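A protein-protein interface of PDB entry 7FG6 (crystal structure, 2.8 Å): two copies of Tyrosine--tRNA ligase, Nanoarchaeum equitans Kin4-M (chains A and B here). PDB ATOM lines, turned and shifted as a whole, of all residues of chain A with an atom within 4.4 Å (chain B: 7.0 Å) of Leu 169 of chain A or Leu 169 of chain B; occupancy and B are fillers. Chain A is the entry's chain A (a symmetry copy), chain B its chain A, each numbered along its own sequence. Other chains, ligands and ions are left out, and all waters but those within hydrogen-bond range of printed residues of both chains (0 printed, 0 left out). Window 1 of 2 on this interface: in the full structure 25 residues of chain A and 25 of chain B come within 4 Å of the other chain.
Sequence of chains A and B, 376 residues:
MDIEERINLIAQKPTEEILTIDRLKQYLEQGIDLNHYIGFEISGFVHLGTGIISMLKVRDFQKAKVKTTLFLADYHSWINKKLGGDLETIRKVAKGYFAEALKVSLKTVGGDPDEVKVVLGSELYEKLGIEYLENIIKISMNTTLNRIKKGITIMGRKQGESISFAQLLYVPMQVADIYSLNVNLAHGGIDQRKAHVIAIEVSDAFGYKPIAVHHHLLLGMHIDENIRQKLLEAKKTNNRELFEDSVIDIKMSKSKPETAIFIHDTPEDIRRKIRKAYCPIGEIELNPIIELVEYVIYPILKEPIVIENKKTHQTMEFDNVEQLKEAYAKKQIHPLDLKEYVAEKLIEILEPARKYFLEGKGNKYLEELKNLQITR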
ATOM      1  N   ILE A 136      -7.666  25.478   1.159  1.00  0.00           N
ATOM      2  CA  ILE A 136      -7.630  26.012   2.519  1.00  0.00           C
ATOM      3  C   ILE A 136      -6.605  25.264   3.359  1.00  0.00           C
ATOM      4  O   ILE A 136      -5.828  25.873   4.107  1.00  0.00           O
ATOM      5  CB  ILE A 136      -9.031  25.951   3.155  1.00  0.00           C
ATOM      6  CG1 ILE A 136      -9.977  26.941   2.473  1.00  0.00           C
ATOM      7  CG2 ILE A 136      -8.957  26.229   4.651  1.00  0.00           C
ATOM      8  CD1 ILE A 136     -11.379  26.921   3.039  1.00  0.00           C
ATOM      9  N   ILE A 137      -6.582  23.936   3.248  1.00  0.00           N
ATOM     10  CA  ILE A 137      -5.653  23.147   4.049  1.00  0.00           C
ATOM     11  C   ILE A 137      -4.224  23.349   3.567  1.00  0.00           C
ATOM     12  O   ILE A 137      -3.286  23.400   4.373  1.00  0.00           O
ATOM     13  CB  ILE A 137      -6.054  21.663   4.027  1.00  0.00           C
ATOM     14  CG1 ILE A 137      -7.449  21.483   4.625  1.00  0.00           C
ATOM     15  CG2 ILE A 137      -5.056  20.832   4.804  1.00  0.00           C
ATOM     16  CD1 ILE A 137      -8.010  20.091   4.460  1.00  0.00           C
ATOM     17  N   PHE A 165     -12.794  31.626  16.226  1.00  0.00           N
ATOM     18  CA  PHE A 165     -11.936  30.862  15.330  1.00  0.00           C
ATOM     19  C   PHE A 165     -12.332  31.028  13.870  1.00  0.00           C
ATOM     20  O   PHE A 165     -11.500  30.803  12.984  1.00  0.00           O
ATOM     21  CB  PHE A 165     -11.944  29.378  15.704  1.00  0.00           C
ATOM     22  CG  PHE A 165     -10.861  28.584  15.029  1.00  0.00           C
ATOM     23  CD1 PHE A 165      -9.551  28.656  15.476  1.00  0.00           C
ATOM     24  CD2 PHE A 165     -11.149  27.781  13.938  1.00  0.00           C
ATOM     25  CE1 PHE A 165      -8.551  27.933  14.853  1.00  0.00           C
ATOM     26  CE2 PHE A 165     -10.151  27.056  13.310  1.00  0.00           C
ATOM     27  CZ  PHE A 165      -8.850  27.132  13.769  1.00  0.00           C
ATOM     28  N   ALA A 166     -13.578  31.424  13.597  1.00  0.00           N
ATOM     29  CA  ALA A 166     -13.985  31.671  12.220  1.00  0.00           C
ATOM     30  C   ALA A 166     -13.302  32.909  11.656  1.00  0.00           C
ATOM     31  O   ALA A 166     -12.966  32.953  10.466  1.00  0.00           O
ATOM     32  CB  ALA A 166     -15.505  31.808  12.136  1.00  0.00           C
ATOM     33  N   GLN A 167     -13.089  33.928  12.494  1.00  0.00           N
ATOM     34  CA  GLN A 167     -12.377  35.117  12.042  1.00  0.00           C
ATOM     35  C   GLN A 167     -10.921  34.809  11.721  1.00  0.00           C
ATOM     36  O   GLN A 167     -10.337  35.434  10.831  1.00  0.00           O
ATOM     37  CB  GLN A 167     -12.470  36.219  13.097  1.00  0.00           C
ATOM     38  CG  GLN A 167     -13.872  36.781  13.275  1.00  0.00           C
ATOM     39  CD  GLN A 167     -14.132  37.272  14.685  1.00  0.00           C
ATOM     40  OE1 GLN A 167     -13.217  37.347  15.506  1.00  0.00           O
ATOM     41  NE2 GLN A 167     -15.382  37.605  14.974  1.00  0.00           N
ATOM     42  N   LEU A 168     -10.315  33.857  12.430  1.00  0.00           N
ATOM     43  CA  LEU A 168      -8.977  33.419  12.053  1.00  0.00           C
ATOM     44  C   LEU A 168      -9.017  32.587  10.779  1.00  0.00           C
ATOM     45  O   LEU A 168      -8.146  32.721   9.912  1.00  0.00           O
ATOM     46  CB  LEU A 168      -8.337  32.635  13.199  1.00  0.00           C
ATOM     47  CG  LEU A 168      -8.015  33.452  14.455  1.00  0.00           C
ATOM     48  CD1 LEU A 168      -7.510  32.554  15.572  1.00  0.00           C
ATOM     49  CD2 LEU A 168      -7.002  34.545  14.145  1.00  0.00           C
ATOM     50  N   LEU A 169     -10.033  31.731  10.640  1.00  0.00           N
ATOM     51  CA  LEU A 169     -10.204  30.950   9.420  1.00  0.00           C
ATOM     52  C   LEU A 169     -10.521  31.833   8.219  1.00  0.00           C
ATOM     53  O   LEU A 169     -10.269  31.425   7.078  1.00  0.00           O
ATOM     54  CB  LEU A 169     -11.303  29.906   9.632  1.00  0.00           C
ATOM     55  CG  LEU A 169     -11.737  29.031   8.455  1.00  0.00           C
ATOM     56  CD1 LEU A 169     -10.647  28.032   8.093  1.00  0.00           C
ATOM     57  CD2 LEU A 169     -13.044  28.317   8.772  1.00  0.00           C
ATOM     58  N   TYR A 170     -11.075  33.027   8.460  1.00  0.00           N
ATOM     59  CA  TYR A 170     -11.254  34.030   7.414  1.00  0.00           C
ATOM     60  C   TYR A 170     -10.028  34.162   6.521  1.00  0.00           C
ATOM     61  O   TYR A 170     -10.160  34.207   5.291  1.00  0.00           O
ATOM     62  CB  TYR A 170     -11.541  35.388   8.049  1.00  0.00           C
ATOM     63  CG  TYR A 170     -11.732  36.509   7.053  1.00  0.00           C
ATOM     64  CD1 TYR A 170     -12.952  36.713   6.437  1.00  0.00           C
ATOM     65  CD2 TYR A 170     -10.669  37.319   6.678  1.00  0.00           C
ATOM     66  CE1 TYR A 170     -13.124  37.732   5.530  1.00  0.00           C
ATOM     67  CE2 TYR A 170     -10.833  38.334   5.756  1.00  0.00           C
ATOM     68  CZ  TYR A 170     -12.067  38.534   5.180  1.00  0.00           C
ATOM     69  OH  TYR A 170     -12.266  39.533   4.256  1.00  0.00           O
ATOM     70  N   VAL A 171      -8.844  34.266   7.116  1.00  0.00           N
ATOM     71  CA  VAL A 171      -7.639  34.654   6.389  1.00  0.00           C
ATOM     72  C   VAL A 171      -7.226  33.570   5.395  1.00  0.00           C
ATOM     73  O   VAL A 171      -7.008  33.892   4.218  1.00  0.00           O
ATOM     74  CB  VAL A 171      -6.496  35.002   7.356  1.00  0.00           C
ATOM     75  CG1 VAL A 171      -5.343  35.642   6.600  1.00  0.00           C
ATOM     76  CG2 VAL A 171      -6.997  35.922   8.459  1.00  0.00           C
ATOM     77  N   PRO A 172      -7.101  32.294   5.788  1.00  0.00           N
ATOM     78  CA  PRO A 172      -6.826  31.269   4.767  1.00  0.00           C
ATOM     79  C   PRO A 172      -7.953  31.116   3.765  1.00  0.00           C
ATOM     80  O   PRO A 172      -7.706  30.700   2.626  1.00  0.00           O
ATOM     81  CB  PRO A 172      -6.623  29.991   5.596  1.00  0.00           C
ATOM     82  CG  PRO A 172      -6.276  30.471   6.959  1.00  0.00           C
ATOM     83  CD  PRO A 172      -7.095  31.706   7.140  1.00  0.00           C
ATOM     84  N   MET A 173      -9.188  31.440   4.156  1.00  0.00           N
ATOM     85  CA  MET A 173     -10.297  31.404   3.209  1.00  0.00           C
ATOM     86  C   MET A 173     -10.134  32.467   2.130  1.00  0.00           C
ATOM     87  O   MET A 173     -10.412  32.213   0.953  1.00  0.00           O
ATOM     88  CB  MET A 173     -11.623  31.589   3.946  1.00  0.00           C
ATOM     89  CG  MET A 173     -12.238  30.302   4.462  1.00  0.00           C
ATOM     90  SD  MET A 173     -13.492  30.600   5.723  1.00  0.00           S
ATOM     91  CE  MET A 173     -14.875  31.117   4.712  1.00  0.00           C
ATOM     92  N   HIS B  76      -7.282  14.466   7.807  1.00  0.00           N
ATOM     93  CA  HIS B  76      -6.676  14.626   9.119  1.00  0.00           C
ATOM     94  C   HIS B  76      -5.286  14.009   9.180  1.00  0.00           C
ATOM     95  O   HIS B  76      -4.412  14.521   9.890  1.00  0.00           O
ATOM     96  CB  HIS B  76      -7.595  14.020  10.172  1.00  0.00           C
ATOM     97  CG  HIS B  76      -8.926  14.702  10.268  1.00  0.00           C
ATOM     98  ND1 HIS B  76      -9.956  14.225  11.049  1.00  0.00           N
ATOM     99  CD2 HIS B  76      -9.388  15.833   9.684  1.00  0.00           C
ATOM    100  CE1 HIS B  76     -10.997  15.034  10.942  1.00  0.00           C
ATOM    101  NE2 HIS B  76     -10.679  16.016  10.119  1.00  0.00           N
ATOM    102  N   ILE B  79      -2.949  16.352   7.104  1.00  0.00           N
ATOM    103  CA  ILE B  79      -2.520  17.536   7.841  1.00  0.00           C
ATOM    104  C   ILE B  79      -1.309  17.209   8.707  1.00  0.00           C
ATOM    105  O   ILE B  79      -0.319  17.950   8.727  1.00  0.00           O
ATOM    106  CB  ILE B  79      -3.682  18.094   8.683  1.00  0.00           C
ATOM    107  CG1 ILE B  79      -4.639  18.898   7.802  1.00  0.00           C
ATOM    108  CG2 ILE B  79      -3.157  18.955   9.823  1.00  0.00           C
ATOM    109  CD1 ILE B  79      -5.934  19.270   8.490  1.00  0.00           C
ATOM    110  N   TYR B 132     -20.646  20.840   4.792  1.00  0.00           N
ATOM    111  CA  TYR B 132     -19.473  20.586   5.623  1.00  0.00           C
ATOM    112  C   TYR B 132     -18.756  21.884   5.973  1.00  0.00           C
ATOM    113  O   TYR B 132     -18.397  22.113   7.134  1.00  0.00           O
ATOM    114  CB  TYR B 132     -18.523  19.621   4.913  1.00  0.00           C
ATOM    115  CG  TYR B 132     -17.310  19.260   5.739  1.00  0.00           C
ATOM    116  CD1 TYR B 132     -17.448  18.659   6.983  1.00  0.00           C
ATOM    117  CD2 TYR B 132     -16.027  19.528   5.279  1.00  0.00           C
ATOM    118  CE1 TYR B 132     -16.343  18.331   7.744  1.00  0.00           C
ATOM    119  CE2 TYR B 132     -14.916  19.201   6.033  1.00  0.00           C
ATOM    120  CZ  TYR B 132     -15.079  18.606   7.266  1.00  0.00           C
ATOM    121  OH  TYR B 132     -13.978  18.278   8.021  1.00  0.00           O
ATOM    122  N   LEU B 133     -18.537  22.749   4.978  1.00  0.00           N
ATOM    123  CA  LEU B 133     -17.887  24.027   5.244  1.00  0.00           C
ATOM    124  C   LEU B 133     -18.746  24.919   6.131  1.00  0.00           C
ATOM    125  O   LEU B 133     -18.212  25.674   6.951  1.00  0.00           O
ATOM    126  CB  LEU B 133     -17.564  24.740   3.931  1.00  0.00           C
ATOM    127  CG  LEU B 133     -16.609  25.932   4.037  1.00  0.00           C
ATOM    128  CD1 LEU B 133     -15.162  25.469   3.969  1.00  0.00           C
ATOM    129  CD2 LEU B 133     -16.900  26.957   2.950  1.00  0.00           C
ATOM    130  N   ILE B 136     -18.275  23.728   9.679  1.00  0.00           N
ATOM    131  CA  ILE B 136     -16.974  24.163  10.182  1.00  0.00           C
ATOM    132  C   ILE B 136     -17.045  25.603  10.672  1.00  0.00           C
ATOM    133  O   ILE B 136     -16.520  25.939  11.741  1.00  0.00           O
ATOM    134  CB  ILE B 136     -15.895  23.991   9.097  1.00  0.00           C
ATOM    135  CG1 ILE B 136     -15.629  22.509   8.832  1.00  0.00           C
ATOM    136  CG2 ILE B 136     -14.608  24.700   9.500  1.00  0.00           C
ATOM    137  CD1 ILE B 136     -14.589  22.267   7.762  1.00  0.00           C
ATOM    138  N   ILE B 137     -17.700  26.473   9.903  1.00  0.00           N
ATOM    139  CA  ILE B 137     -17.780  27.878  10.286  1.00  0.00           C
ATOM    140  C   ILE B 137     -18.688  28.054  11.494  1.00  0.00           C
ATOM    141  O   ILE B 137     -18.417  28.880  12.374  1.00  0.00           O
ATOM    142  CB  ILE B 137     -18.248  28.732   9.096  1.00  0.00           C
ATOM    143  CG1 ILE B 137     -17.252  28.622   7.942  1.00  0.00           C
ATOM    144  CG2 ILE B 137     -18.393  30.181   9.508  1.00  0.00           C
ATOM    145  CD1 ILE B 137     -17.729  29.263   6.660  1.00  0.00           C
ATOM    146  N   SER B 140     -16.584  27.079  14.409  1.00  0.00           N
ATOM    147  CA  SER B 140     -15.545  28.076  14.648  1.00  0.00           C
ATOM    148  C   SER B 140     -16.108  29.399  15.151  1.00  0.00           C
ATOM    149  O   SER B 140     -15.387  30.155  15.812  1.00  0.00           O
ATOM    150  CB  SER B 140     -14.737  28.306  13.371  1.00  0.00           C
ATOM    151  OG  SER B 140     -14.163  27.095  12.905  1.00  0.00           O
ATOM    152  N   ILE B 148      -9.264  25.743  20.989  1.00  0.00           N
ATOM    153  CA  ILE B 148      -8.690  24.988  19.881  1.00  0.00           C
ATOM    154  C   ILE B 148      -7.193  24.794  20.088  1.00  0.00           C
ATOM    155  O   ILE B 148      -6.643  23.727  19.787  1.00  0.00           O
ATOM    156  CB  ILE B 148      -8.996  25.691  18.546  1.00  0.00           C
ATOM    157  CG1 ILE B 148     -10.506  25.865  18.371  1.00  0.00           C
ATOM    158  CG2 ILE B 148      -8.415  24.907  17.386  1.00  0.00           C
ATOM    159  CD1 ILE B 148     -11.279  24.565  18.385  1.00  0.00           C
ATOM    160  N   MET B 155      -4.760  14.821  18.217  1.00  0.00           N
ATOM    161  CA  MET B 155      -3.911  14.166  17.234  1.00  0.00           C
ATOM    162  C   MET B 155      -2.620  13.624  17.833  1.00  0.00           C
ATOM    163  O   MET B 155      -1.794  13.076  17.097  1.00  0.00           O
ATOM    164  CB  MET B 155      -3.580  15.135  16.095  1.00  0.00           C
ATOM    165  CG  MET B 155      -2.763  16.339  16.529  1.00  0.00           C
ATOM    166  SD  MET B 155      -2.582  17.559  15.218  1.00  0.00           S
ATOM    167  CE  MET B 155      -3.855  18.724  15.687  1.00  0.00           C
ATOM    168  N   SER B 164       1.024  24.295  12.838  1.00  0.00           N
ATOM    169  CA  SER B 164       0.562  24.832  11.567  1.00  0.00           C
ATOM    170  C   SER B 164      -0.926  25.102  11.714  1.00  0.00           C
ATOM    171  O   SER B 164      -1.610  24.449  12.507  1.00  0.00           O
ATOM    172  CB  SER B 164       0.830  23.881  10.393  1.00  0.00           C
ATOM    173  OG  SER B 164       0.034  22.713  10.477  1.00  0.00           O
ATOM    174  N   PHE B 165      -1.425  26.082  10.956  1.00  0.00           N
ATOM    175  CA  PHE B 165      -2.828  26.451  11.092  1.00  0.00           C
ATOM    176  C   PHE B 165      -3.764  25.318  10.695  1.00  0.00           C
ATOM    177  O   PHE B 165      -4.923  25.306  11.125  1.00  0.00           O
ATOM    178  CB  PHE B 165      -3.144  27.699  10.266  1.00  0.00           C
ATOM    179  CG  PHE B 165      -4.477  28.311  10.592  1.00  0.00           C
ATOM    180  CD1 PHE B 165      -4.643  29.069  11.740  1.00  0.00           C
ATOM    181  CD2 PHE B 165      -5.568  28.115   9.761  1.00  0.00           C
ATOM    182  CE1 PHE B 165      -5.870  29.629  12.048  1.00  0.00           C
ATOM    183  CE2 PHE B 165      -6.798  28.671  10.065  1.00  0.00           C
ATOM    184  CZ  PHE B 165      -6.948  29.430  11.210  1.00  0.00           C
ATOM    185  N   ALA B 166      -3.290  24.362   9.892  1.00  0.00           N
ATOM    186  CA  ALA B 166      -4.121  23.217   9.542  1.00  0.00           C
ATOM    187  C   ALA B 166      -4.345  22.312  10.745  1.00  0.00           C
ATOM    188  O   ALA B 166      -5.426  21.728  10.897  1.00  0.00           O
ATOM    189  CB  ALA B 166      -3.487  22.437   8.391  1.00  0.00           C
ATOM    190  N   GLN B 167      -3.337  22.179  11.610  1.00  0.00           N
ATOM    191  CA  GLN B 167      -3.505  21.385  12.821  1.00  0.00           C
ATOM    192  C   GLN B 167      -4.508  22.021  13.773  1.00  0.00           C
ATOM    193  O   GLN B 167      -5.210  21.310  14.499  1.00  0.00           O
ATOM    194  CB  GLN B 167      -2.156  21.193  13.516  1.00  0.00           C
ATOM    195  CG  GLN B 167      -1.185  20.319  12.738  1.00  0.00           C
ATOM    196  CD  GLN B 167       0.263  20.690  12.986  1.00  0.00           C
ATOM    197  OE1 GLN B 167       0.568  21.498  13.864  1.00  0.00           O
ATOM    198  NE2 GLN B 167       1.165  20.103  12.209  1.00  0.00           N
ATOM    199  N   LEU B 168      -4.593  23.351  13.791  1.00  0.00           N
ATOM    200  CA  LEU B 168      -5.646  23.996  14.566  1.00  0.00           C
ATOM    201  C   LEU B 168      -7.001  23.816  13.895  1.00  0.00           C
ATOM    202  O   LEU B 168      -8.010  23.581  14.568  1.00  0.00           O
ATOM    203  CB  LEU B 168      -5.323  25.477  14.761  1.00  0.00           C
ATOM    204  CG  LEU B 168      -4.110  25.775  15.647  1.00  0.00           C
ATOM    205  CD1 LEU B 168      -3.801  27.262  15.665  1.00  0.00           C
ATOM    206  CD2 LEU B 168      -4.331  25.255  17.061  1.00  0.00           C
ATOM    207  N   LEU B 169      -7.039  23.907  12.563  1.00  0.00           N
ATOM    208  CA  LEU B 169      -8.274  23.668  11.823  1.00  0.00           C
ATOM    209  C   LEU B 169      -8.736  22.220  11.938  1.00  0.00           C
ATOM    210  O   LEU B 169      -9.930  21.946  11.766  1.00  0.00           O
ATOM    211  CB  LEU B 169      -8.075  24.061  10.357  1.00  0.00           C
ATOM    212  CG  LEU B 169      -9.202  23.803   9.356  1.00  0.00           C
ATOM    213  CD1 LEU B 169     -10.372  24.743   9.607  1.00  0.00           C
ATOM    214  CD2 LEU B 169      -8.692  23.938   7.928  1.00  0.00           C
ATOM    215  N   TYR B 170      -7.809  21.298  12.218  1.00  0.00           N
ATOM    216  CA  TYR B 170      -8.153  19.914  12.532  1.00  0.00           C
ATOM    217  C   TYR B 170      -9.335  19.814  13.487  1.00  0.00           C
ATOM    218  O   TYR B 170     -10.250  19.011  13.260  1.00  0.00           O
ATOM    219  CB  TYR B 170      -6.954  19.217  13.170  1.00  0.00           C
ATOM    220  CG  TYR B 170      -7.205  17.776  13.549  1.00  0.00           C
ATOM    221  CD1 TYR B 170      -7.098  16.765  12.615  1.00  0.00           C
ATOM    222  CD2 TYR B 170      -7.618  17.439  14.831  1.00  0.00           C
ATOM    223  CE1 TYR B 170      -7.328  15.454  12.960  1.00  0.00           C
ATOM    224  CE2 TYR B 170      -7.866  16.125  15.180  1.00  0.00           C
ATOM    225  CZ  TYR B 170      -7.721  15.133  14.235  1.00  0.00           C
ATOM    226  OH  TYR B 170      -7.963  13.816  14.546  1.00  0.00           O
ATOM    227  N   VAL B 171      -9.315  20.583  14.571  1.00  0.00           N
ATOM    228  CA  VAL B 171     -10.249  20.393  15.678  1.00  0.00           C
ATOM    229  C   VAL B 171     -11.674  20.742  15.258  1.00  0.00           C
ATOM    230  O   VAL B 171     -12.579  19.923  15.480  1.00  0.00           O
ATOM    231  CB  VAL B 171      -9.810  21.193  16.916  1.00  0.00           C
ATOM    232  CG1 VAL B 171     -10.638  20.788  18.124  1.00  0.00           C
ATOM    233  CG2 VAL B 171      -8.327  20.985  17.183  1.00  0.00           C
ATOM    234  N   PRO B 172     -11.946  21.912  14.663  1.00  0.00           N
ATOM    235  CA  PRO B 172     -13.311  22.146  14.164  1.00  0.00           C
ATOM    236  C   PRO B 172     -13.703  21.198  13.047  1.00  0.00           C
ATOM    237  O   PRO B 172     -14.897  20.927  12.866  1.00  0.00           O
ATOM    238  CB  PRO B 172     -13.264  23.604  13.681  1.00  0.00           C
ATOM    239  CG  PRO B 172     -12.115  24.210  14.404  1.00  0.00           C
ATOM    240  CD  PRO B 172     -11.107  23.112  14.488  1.00  0.00           C
ATOM    241  N   MET B 173     -12.730  20.684  12.291  1.00  0.00           N
ATOM    242  CA  MET B 173     -13.036  19.693  11.265  1.00  0.00           C
ATOM    243  C   MET B 173     -13.528  18.392  11.886  1.00  0.00           C
ATOM    244  O   MET B 173     -14.463  17.767  11.372  1.00  0.00           O
ATOM    245  CB  MET B 173     -11.805  19.439  10.396  1.00  0.00           C
ATOM    246  CG  MET B 173     -11.668  20.381   9.213  1.00  0.00           C
ATOM    247  SD  MET B 173      -9.998  20.384   8.533  1.00  0.00           S
ATOM    248  CE  MET B 173     -10.009  18.856   7.599  1.00  0.00           C
ATOM    249  N   GLN B 174     -12.908  17.968  12.990  1.00  0.00           N
ATOM    250  CA  GLN B 174     -13.358  16.758  13.671  1.00  0.00           C
ATOM    251  C   GLN B 174     -14.739  16.951  14.284  1.00  0.00           C
ATOM    252  O   GLN B 174     -15.581  16.048  14.229  1.00  0.00           O
ATOM    253  CB  GLN B 174     -12.346  16.349  14.740  1.00  0.00           C
ATOM    254  CG  GLN B 174     -12.790  15.173  15.595  1.00  0.00           C
ATOM    255  CD  GLN B 174     -11.633  14.499  16.304  1.00  0.00           C
ATOM    256  OE1 GLN B 174     -10.490  14.573  15.856  1.00  0.00           O
ATOM    257  NE2 GLN B 174     -11.925  13.838  17.417  1.00  0.00           N
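Printed residues of chain B within 4 Å of Leu 168 of chain A: Phe 165. Printed residues of chain B within 4 Å of Leu 169 of chain A: Phe 165 (3.9 Å) and Leu 169 (3.6 Å). Of the printed residues of chain A, Ile 148 of chain B touches Phe 165. Met 155 of chain B touches none of the printed residues of chain A. Of the printed residues of chain A, Leu 169 of chain B touches Phe 165 and Leu 169. Of the printed residues of chain A, Pro 172 of chain B touches Phe 165. The nearest printed residue of chain A that does not touch Leu 169 of chain B is Ile 136 of chain A (4.01 Å). The nearest printed residue of chain B that does not touch Phe 165 of chain A is Ile 136 of chain B (6.1 Å).
O of Ser 140 of chain B lies within hydrogen-bond range of N of Phe 165 of chain A (3.0 Å). The backbone NH (N) of Ala 166 of chain A lies within hydrogen-bond range of the backbone carbonyl oxygen (O) of Ser 140 of chain B.
Ile 137 of chain A touches Met 173 of chain B, and with the chains exchanged Met 173 of chain A touches Ile 137 of chain B. Phe 165 of chain B touches its own counterpart, Phe 165 of chain A. Phe 165 of chain A touches Leu 169 of chain B, and with the chains exchanged Leu 169 of chain A touches Phe 165 of chain B. Phe 165 of chain A touches Pro 172 of chain B, and with the chains exchanged Pro 172 of chain A touches Phe 165 of chain B. 11 positions are printed for both chains. Of the 14 pairs that touch across the chains among the printed residues, 10 have their exchanged pair printed and touching as well.
Hydrophobic or aromatic side chains of chain A that line the printed part of chain B: Ile 137, Phe 165, Ala 166, Leu 169, Pro 172 and Met 173.
The backbone carbonyl oxygen (O) of Met 173 of chain B sits close to the side-chain hydroxyl (OH) of Tyr 132 of chain B (3.4 Å). OG of Ser 140 of chain B is in hydrogen-bond range of O of Ile 136 of chain B.
Among the printed residues, merely in contact across the chains: Ile 137 of chain A with Ile 79 of chain B (3.6 Å), Ile 137 of chain A with Met 173 of chain B (3.9 Å), Phe 165 of chain A with Ile 148 of chain B (3.9 Å), Phe 165 of chain A with Phe 165 of chain B (3.9 Å), Phe 165 of chain A with Leu 168 of chain B (3.7 Å), Phe 165 of chain A with Leu 169 of chain B (3.9 Å), Phe 165 of chain A with Pro 172 of chain B (3.6 Å), Leu 168 of chain A with Phe 165 of chain B (3.7 Å), Leu 169 of chain A with Phe 165 of chain B (3.9 Å), Leu 169 of chain A with Leu 169 of chain B (3.6 Å), Pro 172 of chain A with Phe 165 of chain B (3.6 Å) and Met 173 of chain A with Ile 137 of chain B (3.9 Å).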
